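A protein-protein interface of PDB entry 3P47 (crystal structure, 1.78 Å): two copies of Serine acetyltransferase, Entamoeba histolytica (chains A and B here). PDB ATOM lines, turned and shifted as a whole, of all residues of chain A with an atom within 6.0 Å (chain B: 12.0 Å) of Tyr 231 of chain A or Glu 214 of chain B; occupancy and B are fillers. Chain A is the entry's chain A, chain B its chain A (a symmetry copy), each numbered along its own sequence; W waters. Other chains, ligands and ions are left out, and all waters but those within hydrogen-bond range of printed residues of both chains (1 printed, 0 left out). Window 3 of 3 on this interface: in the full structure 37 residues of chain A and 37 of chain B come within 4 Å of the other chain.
The backbone carbonyl oxygen (O) of Val 232 of chain A lies close to the side-chain amide oxygen (OE1) of Gln 212 of chain B, at 3.3 Å. OG1 of Thr 233 of chain A is in hydrogen-bond range of OE1 of Gln 212 of chain B. The backbone carbonyl oxygen of Gln 212 of chain B is in hydrogen-bond range of the guanidinium group of Arg 251 of chain A (2.9 Å). The backbone carbonyl oxygen of Trp 197 of chain A lies close to the side-chain amide oxygen of Gln 212 of chain B, at 2.9 Å.
The backbone NH (N) of Thr 233 of chain A is in hydrogen-bond range of the backbone carbonyl oxygen (O) of Val 250 of chain A (3.0 Å). The backbone NH (N) of Tyr 231 of chain A lies close to the backbone carbonyl oxygen (O) of Trp 197 of chain A (3.5 Å). The backbone carbonyl oxygen (O) of Glu 196 of chain A sits at hydrogen-bond distance from the backbone NH (N) of Tyr 231 of chain A. The side-chain sulfur (SG) of Cys 198 of chain A lies close to the backbone carbonyl oxygen (O) of Val 232 of chain A, at 3.7 Å. N of Val 232 of chain A sits at hydrogen-bond distance from O of Trp 197 of chain A (3.4 Å).
Among the printed residues, merely in contact across the chains: Tyr 231 of chain A with Gln 212 of chain B (3.6 Å), Tyr 231 of chain A with Glu 214 of chain B (3.98 Å), Thr 233 of chain A with His 210 of chain B (3.7 Å), Thr 233 of chain A with Phe 211 of chain B (3.7 Å) and Arg 251 of chain A with Phe 211 of chain B (3.6 Å).
No residue of chain B comes within 4 Å of Gly 195 of chain A. Trp 197 of chain A touches just one residue of chain B: Gln 212. Cys 198 of chain A touches none of the printed residues of chain B. No residue of chain B comes within 4 Å of Gly 229 of chain A. Of chain B, only Gln 212 comes within 4 Å of Val 232 of chain A. Thr 233 of chain A touches three residues of chain B. Of the printed residues of chain A, Phe 211 of chain B touches Thr 233 (3.7 Å) and Arg 251 (3.6 Å). Printed residues of chain A within 4 Å of Gln 212 of chain B: Trp 197 (2.9 Å), Tyr 231 (3.6 Å), Val 232 (3.3 Å), Thr 233 (3.1 Å) and Arg 251 (2.9 Å). Of the printed residues of chain A, Glu 214 of chain B touches Tyr 231. Val 217 of chain B touches none of the printed residues of chain A. The nearest printed residue of chain B that does not touch Tyr 231 of chain A is Gly 215 of chain B (4.2 Å). The nearest printed residue of chain A that does not touch Glu 214 of chain B is His 249 of chain A (5.1 Å).
Hydrophobic or aromatic side chains of chain A within 4 Å of the printed part of chain B: Trp 197 and Tyr 231. Among the printed residues, no Asp or Glu carboxylate lies within 4 Å of a Lys or Arg side-chain nitrogen of the other chain.
No position is printed for both chains.
Water W1 bridges O of Glu 214 of chain B (2.9 Å) and NE2 of His 249 of chain A (3.4 Å).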
ATOM      1  N   GLY A 195     -12.831  38.997 -24.142  1.00  0.00           N
ATOM      2  CA  GLY A 195     -12.956  38.841 -22.692  1.00  0.00           C
ATOM      3  C   GLY A 195     -11.614  38.628 -22.015  1.00  0.00           C
ATOM      4  O   GLY A 195     -10.554  38.896 -22.603  1.00  0.00           O
ATOM      5  N   GLU A 196     -11.661  38.111 -20.783  1.00  0.00           N
ATOM      6  CA  GLU A 196     -10.478  37.987 -19.930  1.00  0.00           C
ATOM      7  C   GLU A 196      -9.666  36.744 -20.325  1.00  0.00           C
ATOM      8  O   GLU A 196     -10.215  35.758 -20.849  1.00  0.00           O
ATOM      9  CB  GLU A 196     -10.914  37.870 -18.444  1.00  0.00           C
ATOM     10  CG  GLU A 196      -9.828  38.189 -17.413  1.00  0.00           C
ATOM     11  CD  GLU A 196      -9.660  39.676 -17.068  1.00  0.00           C
ATOM     12  OE1 GLU A 196      -8.660  40.015 -16.389  1.00  0.00           O
ATOM     13  OE2 GLU A 196     -10.503  40.511 -17.462  1.00  0.00           O
ATOM     14  N   TRP A 197      -8.361  36.778 -20.053  1.00  0.00           N
ATOM     15  CA  TRP A 197      -7.514  35.599 -20.314  1.00  0.00           C
ATOM     16  C   TRP A 197      -7.657  35.111 -21.753  1.00  0.00           C
ATOM     17  O   TRP A 197      -7.867  33.906 -22.017  1.00  0.00           O
ATOM     18  CB  TRP A 197      -7.850  34.462 -19.326  1.00  0.00           C
ATOM     19  CG  TRP A 197      -7.152  34.625 -18.015  1.00  0.00           C
ATOM     20  CD1 TRP A 197      -7.691  35.043 -16.838  1.00  0.00           C
ATOM     21  CD2 TRP A 197      -5.776  34.359 -17.764  1.00  0.00           C
ATOM     22  NE1 TRP A 197      -6.725  35.060 -15.852  1.00  0.00           N
ATOM     23  CE2 TRP A 197      -5.543  34.623 -16.398  1.00  0.00           C
ATOM     24  CE3 TRP A 197      -4.715  33.875 -18.561  1.00  0.00           C
ATOM     25  CZ2 TRP A 197      -4.282  34.478 -15.809  1.00  0.00           C
ATOM     26  CZ3 TRP A 197      -3.445  33.745 -17.978  1.00  0.00           C
ATOM     27  CH2 TRP A 197      -3.253  34.034 -16.605  1.00  0.00           C
ATOM     28  N   CYS A 198      -7.547  36.045 -22.708  1.00  0.00           N
ATOM     29  CA  CYS A 198      -7.435  35.640 -24.095  1.00  0.00           C
ATOM     30  C   CYS A 198      -5.970  35.466 -24.479  1.00  0.00           C
ATOM     31  O   CYS A 198      -5.158  36.333 -24.192  1.00  0.00           O
ATOM     32  CB  CYS A 198      -8.144  36.661 -25.017  1.00  0.00           C
ATOM     33  SG  CYS A 198      -8.280  36.052 -26.706  1.00  0.00           S
ATOM     34  N   GLY A 229     -15.346  35.311 -25.630  1.00  0.00           N
ATOM     35  CA  GLY A 229     -15.579  35.243 -24.188  1.00  0.00           C
ATOM     36  C   GLY A 229     -14.278  35.144 -23.420  1.00  0.00           C
ATOM     37  O   GLY A 229     -13.249  35.692 -23.852  1.00  0.00           O
ATOM     38  N   ASP A 230     -14.314  34.452 -22.274  1.00  0.00           N
ATOM     39  CA  ASP A 230     -13.159  34.357 -21.407  1.00  0.00           C
ATOM     40  C   ASP A 230     -12.425  33.040 -21.600  1.00  0.00           C
ATOM     41  O   ASP A 230     -13.001  32.069 -22.074  1.00  0.00           O
ATOM     42  CB  ASP A 230     -13.553  34.507 -19.921  1.00  0.00           C
ATOM     43  CG  ASP A 230     -14.310  35.802 -19.617  1.00  0.00           C
ATOM     44  OD1 ASP A 230     -14.029  36.867 -20.216  1.00  0.00           O
ATOM     45  OD2 ASP A 230     -15.186  35.762 -18.714  1.00  0.00           O
ATOM     46  N   TYR A 231     -11.146  33.022 -21.227  1.00  0.00           N
ATOM     47  CA  TYR A 231     -10.290  31.827 -21.341  1.00  0.00           C
ATOM     48  C   TYR A 231     -10.306  31.181 -22.720  1.00  0.00           C
ATOM     49  O   TYR A 231     -10.452  29.964 -22.846  1.00  0.00           O
ATOM     50  CB  TYR A 231     -10.603  30.791 -20.242  1.00  0.00           C
ATOM     51  CG  TYR A 231     -10.392  31.353 -18.868  1.00  0.00           C
ATOM     52  CD1 TYR A 231      -9.129  31.310 -18.267  1.00  0.00           C
ATOM     53  CD2 TYR A 231     -11.437  31.961 -18.166  1.00  0.00           C
ATOM     54  CE1 TYR A 231      -8.918  31.831 -17.002  1.00  0.00           C
ATOM     55  CE2 TYR A 231     -11.222  32.507 -16.877  1.00  0.00           C
ATOM     56  CZ  TYR A 231      -9.948  32.434 -16.317  1.00  0.00           C
ATOM     57  OH  TYR A 231      -9.682  32.953 -15.057  1.00  0.00           O
ATOM     58  N   VAL A 232     -10.144  32.019 -23.747  1.00  0.00           N
ATOM     59  CA  VAL A 232     -10.153  31.554 -25.126  1.00  0.00           C
ATOM     60  C   VAL A 232      -8.727  31.602 -25.641  1.00  0.00           C
ATOM     61  O   VAL A 232      -8.026  32.595 -25.422  1.00  0.00           O
ATOM     62  CB  VAL A 232     -11.018  32.459 -26.001  1.00  0.00           C
ATOM     63  CG1 VAL A 232     -10.912  32.069 -27.473  1.00  0.00           C
ATOM     64  CG2 VAL A 232     -12.481  32.400 -25.511  1.00  0.00           C
ATOM     65  N   THR A 233      -8.320  30.529 -26.300  1.00  0.00           N
ATOM     66  CA  THR A 233      -6.994  30.443 -26.963  1.00  0.00           C
ATOM     67  C   THR A 233      -7.194  30.291 -28.454  1.00  0.00           C
ATOM     68  O   THR A 233      -7.895  29.372 -28.936  1.00  0.00           O
ATOM     69  CB  THR A 233      -6.145  29.264 -26.420  1.00  0.00           C
ATOM     70  OG1 THR A 233      -6.104  29.335 -25.002  1.00  0.00           O
ATOM     71  CG2 THR A 233      -4.717  29.308 -26.948  1.00  0.00           C
ATOM     72  N   SER A 248     -16.913  31.182 -23.923  1.00  0.00           N
ATOM     73  CA  SER A 248     -15.812  31.019 -23.004  1.00  0.00           C
ATOM     74  C   SER A 248     -15.201  29.617 -23.070  1.00  0.00           C
ATOM     75  O   SER A 248     -15.841  28.679 -23.552  1.00  0.00           O
ATOM     76  CB  SER A 248     -16.265  31.404 -21.582  1.00  0.00           C
ATOM     77  OG  SER A 248     -16.453  32.822 -21.517  1.00  0.00           O
ATOM     78  N   HIS A 249     -13.938  29.494 -22.659  1.00  0.00           N
ATOM     79  CA  HIS A 249     -13.233  28.213 -22.630  1.00  0.00           C
ATOM     80  C   HIS A 249     -13.229  27.498 -23.987  1.00  0.00           C
ATOM     81  O   HIS A 249     -13.556  26.298 -24.087  1.00  0.00           O
ATOM     82  CB  HIS A 249     -13.825  27.319 -21.506  1.00  0.00           C
ATOM     83  CG  HIS A 249     -13.662  27.908 -20.139  1.00  0.00           C
ATOM     84  ND1 HIS A 249     -14.677  28.571 -19.488  1.00  0.00           N
ATOM     85  CD2 HIS A 249     -12.584  27.975 -19.321  1.00  0.00           C
ATOM     86  CE1 HIS A 249     -14.238  29.011 -18.323  1.00  0.00           C
ATOM     87  NE2 HIS A 249     -12.974  28.649 -18.191  1.00  0.00           N
ATOM     88  N   VAL A 250     -12.902  28.246 -25.046  1.00  0.00           N
ATOM     89  CA  VAL A 250     -12.859  27.678 -26.387  1.00  0.00           C
ATOM     90  C   VAL A 250     -11.391  27.641 -26.777  1.00  0.00           C
ATOM     91  O   VAL A 250     -10.642  28.578 -26.448  1.00  0.00           O
ATOM     92  CB  VAL A 250     -13.702  28.490 -27.396  1.00  0.00           C
ATOM     93  CG1 VAL A 250     -13.364  28.121 -28.851  1.00  0.00           C
ATOM     94  CG2 VAL A 250     -15.212  28.235 -27.143  1.00  0.00           C
ATOM     95  N   ARG A 251     -10.988  26.551 -27.418  1.00  0.00           N
ATOM     96  CA  ARG A 251      -9.650  26.432 -28.037  1.00  0.00           C
ATOM     97  C   ARG A 251      -9.806  26.340 -29.551  1.00  0.00           C
ATOM     98  O   ARG A 251     -10.462  25.436 -30.062  1.00  0.00           O
ATOM     99  CB  ARG A 251      -8.922  25.198 -27.522  1.00  0.00           C
ATOM    100  CG  ARG A 251      -8.812  25.102 -26.007  1.00  0.00           C
ATOM    101  CD  ARG A 251      -8.637  23.645 -25.555  1.00  0.00           C
ATOM    102  NE  ARG A 251      -8.254  23.623 -24.146  1.00  0.00           N
ATOM    103  CZ  ARG A 251      -7.522  22.687 -23.548  1.00  0.00           C
ATOM    104  NH1 ARG A 251      -7.060  21.636 -24.217  1.00  0.00           N
ATOM    105  NH2 ARG A 251      -7.249  22.818 -22.257  1.00  0.00           N
ATOM    106  N   HIS B 210      -0.045  26.711 -27.013  1.00  0.00           N
ATOM    107  CA  HIS B 210      -0.368  26.187 -25.701  1.00  0.00           C
ATOM    108  C   HIS B 210      -1.792  26.577 -25.302  1.00  0.00           C
ATOM    109  O   HIS B 210      -2.045  27.717 -24.918  1.00  0.00           O
ATOM    110  CB  HIS B 210       0.651  26.688 -24.669  1.00  0.00           C
ATOM    111  CG  HIS B 210       2.075  26.458 -25.084  1.00  0.00           C
ATOM    112  ND1 HIS B 210       2.607  25.197 -25.222  1.00  0.00           N
ATOM    113  CD2 HIS B 210       3.059  27.324 -25.421  1.00  0.00           C
ATOM    114  CE1 HIS B 210       3.870  25.294 -25.619  1.00  0.00           C
ATOM    115  NE2 HIS B 210       4.171  26.577 -25.737  1.00  0.00           N
ATOM    116  N   PHE B 211      -2.703  25.619 -25.423  1.00  0.00           N
ATOM    117  CA  PHE B 211      -4.081  25.781 -24.962  1.00  0.00           C
ATOM    118  C   PHE B 211      -4.139  25.932 -23.446  1.00  0.00           C
ATOM    119  O   PHE B 211      -3.531  25.151 -22.699  1.00  0.00           O
ATOM    120  CB  PHE B 211      -4.934  24.577 -25.386  1.00  0.00           C
ATOM    121  CG  PHE B 211      -5.237  24.515 -26.860  1.00  0.00           C
ATOM    122  CD1 PHE B 211      -5.254  25.666 -27.644  1.00  0.00           C
ATOM    123  CD2 PHE B 211      -5.546  23.291 -27.458  1.00  0.00           C
ATOM    124  CE1 PHE B 211      -5.525  25.600 -28.992  1.00  0.00           C
ATOM    125  CE2 PHE B 211      -5.836  23.201 -28.823  1.00  0.00           C
ATOM    126  CZ  PHE B 211      -5.832  24.355 -29.597  1.00  0.00           C
ATOM    127  N   GLN B 212      -4.889  26.942 -22.993  1.00  0.00           N
ATOM    128  CA  GLN B 212      -4.977  27.262 -21.564  1.00  0.00           C
ATOM    129  C   GLN B 212      -5.466  26.102 -20.707  1.00  0.00           C
ATOM    130  O   GLN B 212      -6.386  25.368 -21.085  1.00  0.00           O
ATOM    131  CB  GLN B 212      -5.871  28.473 -21.342  1.00  0.00           C
ATOM    132  CG  GLN B 212      -5.167  29.772 -21.700  1.00  0.00           C
ATOM    133  CD  GLN B 212      -6.106  30.943 -21.699  1.00  0.00           C
ATOM    134  OE1 GLN B 212      -6.620  31.363 -22.757  1.00  0.00           O
ATOM    135  NE2 GLN B 212      -6.367  31.472 -20.502  1.00  0.00           N
ATOM    136  N   GLU B 213      -4.870  25.978 -19.530  1.00  0.00           N
ATOM    137  CA  GLU B 213      -5.108  24.804 -18.719  1.00  0.00           C
ATOM    138  C   GLU B 213      -5.954  24.992 -17.482  1.00  0.00           C
ATOM    139  O   GLU B 213      -6.413  23.989 -16.922  1.00  0.00           O
ATOM    140  CB  GLU B 213      -3.796  24.139 -18.347  1.00  0.00           C
ATOM    141  CG  GLU B 213      -3.254  23.252 -19.446  1.00  0.00           C
ATOM    142  CD  GLU B 213      -1.855  22.833 -19.151  1.00  0.00           C
ATOM    143  OE1 GLU B 213      -0.946  23.706 -19.206  1.00  0.00           O
ATOM    144  OE2 GLU B 213      -1.645  21.622 -18.839  1.00  0.00           O
ATOM    145  N   GLU B 214      -6.156  26.235 -17.037  1.00  0.00           N
ATOM    146  CA  GLU B 214      -6.951  26.462 -15.808  1.00  0.00           C
ATOM    147  C   GLU B 214      -7.462  27.894 -15.527  1.00  0.00           C
ATOM    148  O   GLU B 214      -8.684  28.122 -15.567  1.00  0.00           O
ATOM    149  CB  GLU B 214      -6.236  25.883 -14.564  1.00  0.00           C
ATOM    150  N   GLY B 215      -6.566  28.858 -15.281  1.00  0.00           N
ATOM    151  CA  GLY B 215      -5.141  28.745 -15.604  1.00  0.00           C
ATOM    152  C   GLY B 215      -4.171  28.440 -14.480  1.00  0.00           C
ATOM    153  O   GLY B 215      -4.397  28.837 -13.328  1.00  0.00           O
ATOM    154  N   GLY B 216      -3.127  27.688 -14.833  1.00  0.00           N
ATOM    155  CA  GLY B 216      -1.899  27.532 -14.044  1.00  0.00           C
ATOM    156  C   GLY B 216      -0.812  28.352 -14.742  1.00  0.00           C
ATOM    157  O   GLY B 216      -1.123  29.261 -15.498  1.00  0.00           O
ATOM    158  N   VAL B 217       0.452  28.035 -14.470  1.00  0.00           N
ATOM    159  CA  VAL B 217       1.608  28.708 -15.069  1.00  0.00           C
ATOM    160  C   VAL B 217       2.434  27.641 -15.803  1.00  0.00           C
ATOM    161  O   VAL B 217       3.013  26.738 -15.173  1.00  0.00           O
ATOM    162  CB  VAL B 217       2.488  29.403 -14.011  1.00  0.00           C
ATOM    163  CG1 VAL B 217       3.694  30.036 -14.666  1.00  0.00           C
ATOM    164  CG2 VAL B 217       1.698  30.453 -13.212  1.00  0.00           C
ATOM    165  N   ILE B 218       2.485  27.759 -17.125  1.00  0.00           N
ATOM    166  CA  ILE B 218       3.020  26.694 -17.976  1.00  0.00           C
ATOM    167  C   ILE B 218       4.453  26.396 -17.596  1.00  0.00           C
ATOM    168  O   ILE B 218       5.185  27.290 -17.201  1.00  0.00           O
ATOM    169  CB  ILE B 218       2.905  27.020 -19.479  1.00  0.00           C
ATOM    170  CG1 ILE B 218       3.027  25.741 -20.322  1.00  0.00           C
ATOM    171  CG2 ILE B 218       3.928  28.105 -19.911  1.00  0.00           C
ATOM    172  CD1 ILE B 218       2.465  25.914 -21.754  1.00  0.00           C
ATOM    173  N   LYS B 219       4.822  25.122 -17.686  1.00  0.00           N
ATOM    174  CA  LYS B 219       6.183  24.671 -17.413  1.00  0.00           C
ATOM    175  C   LYS B 219       7.160  25.484 -18.245  1.00  0.00           C
ATOM    176  O   LYS B 219       6.885  25.751 -19.422  1.00  0.00           O
ATOM    177  CB  LYS B 219       6.305  23.207 -17.832  1.00  0.00           C
ATOM    178  CG  LYS B 219       7.756  22.681 -17.838  1.00  0.00           C
ATOM    179  CD  LYS B 219       7.762  21.159 -17.986  1.00  0.00           C
ATOM    180  CE  LYS B 219       7.473  20.708 -19.396  1.00  0.00           C
ATOM    181  NZ  LYS B 219       6.056  20.819 -19.814  1.00  0.00           N
HETATM  182  O   HOH W   1     -11.458  28.816 -15.119  1.00  0.00           O
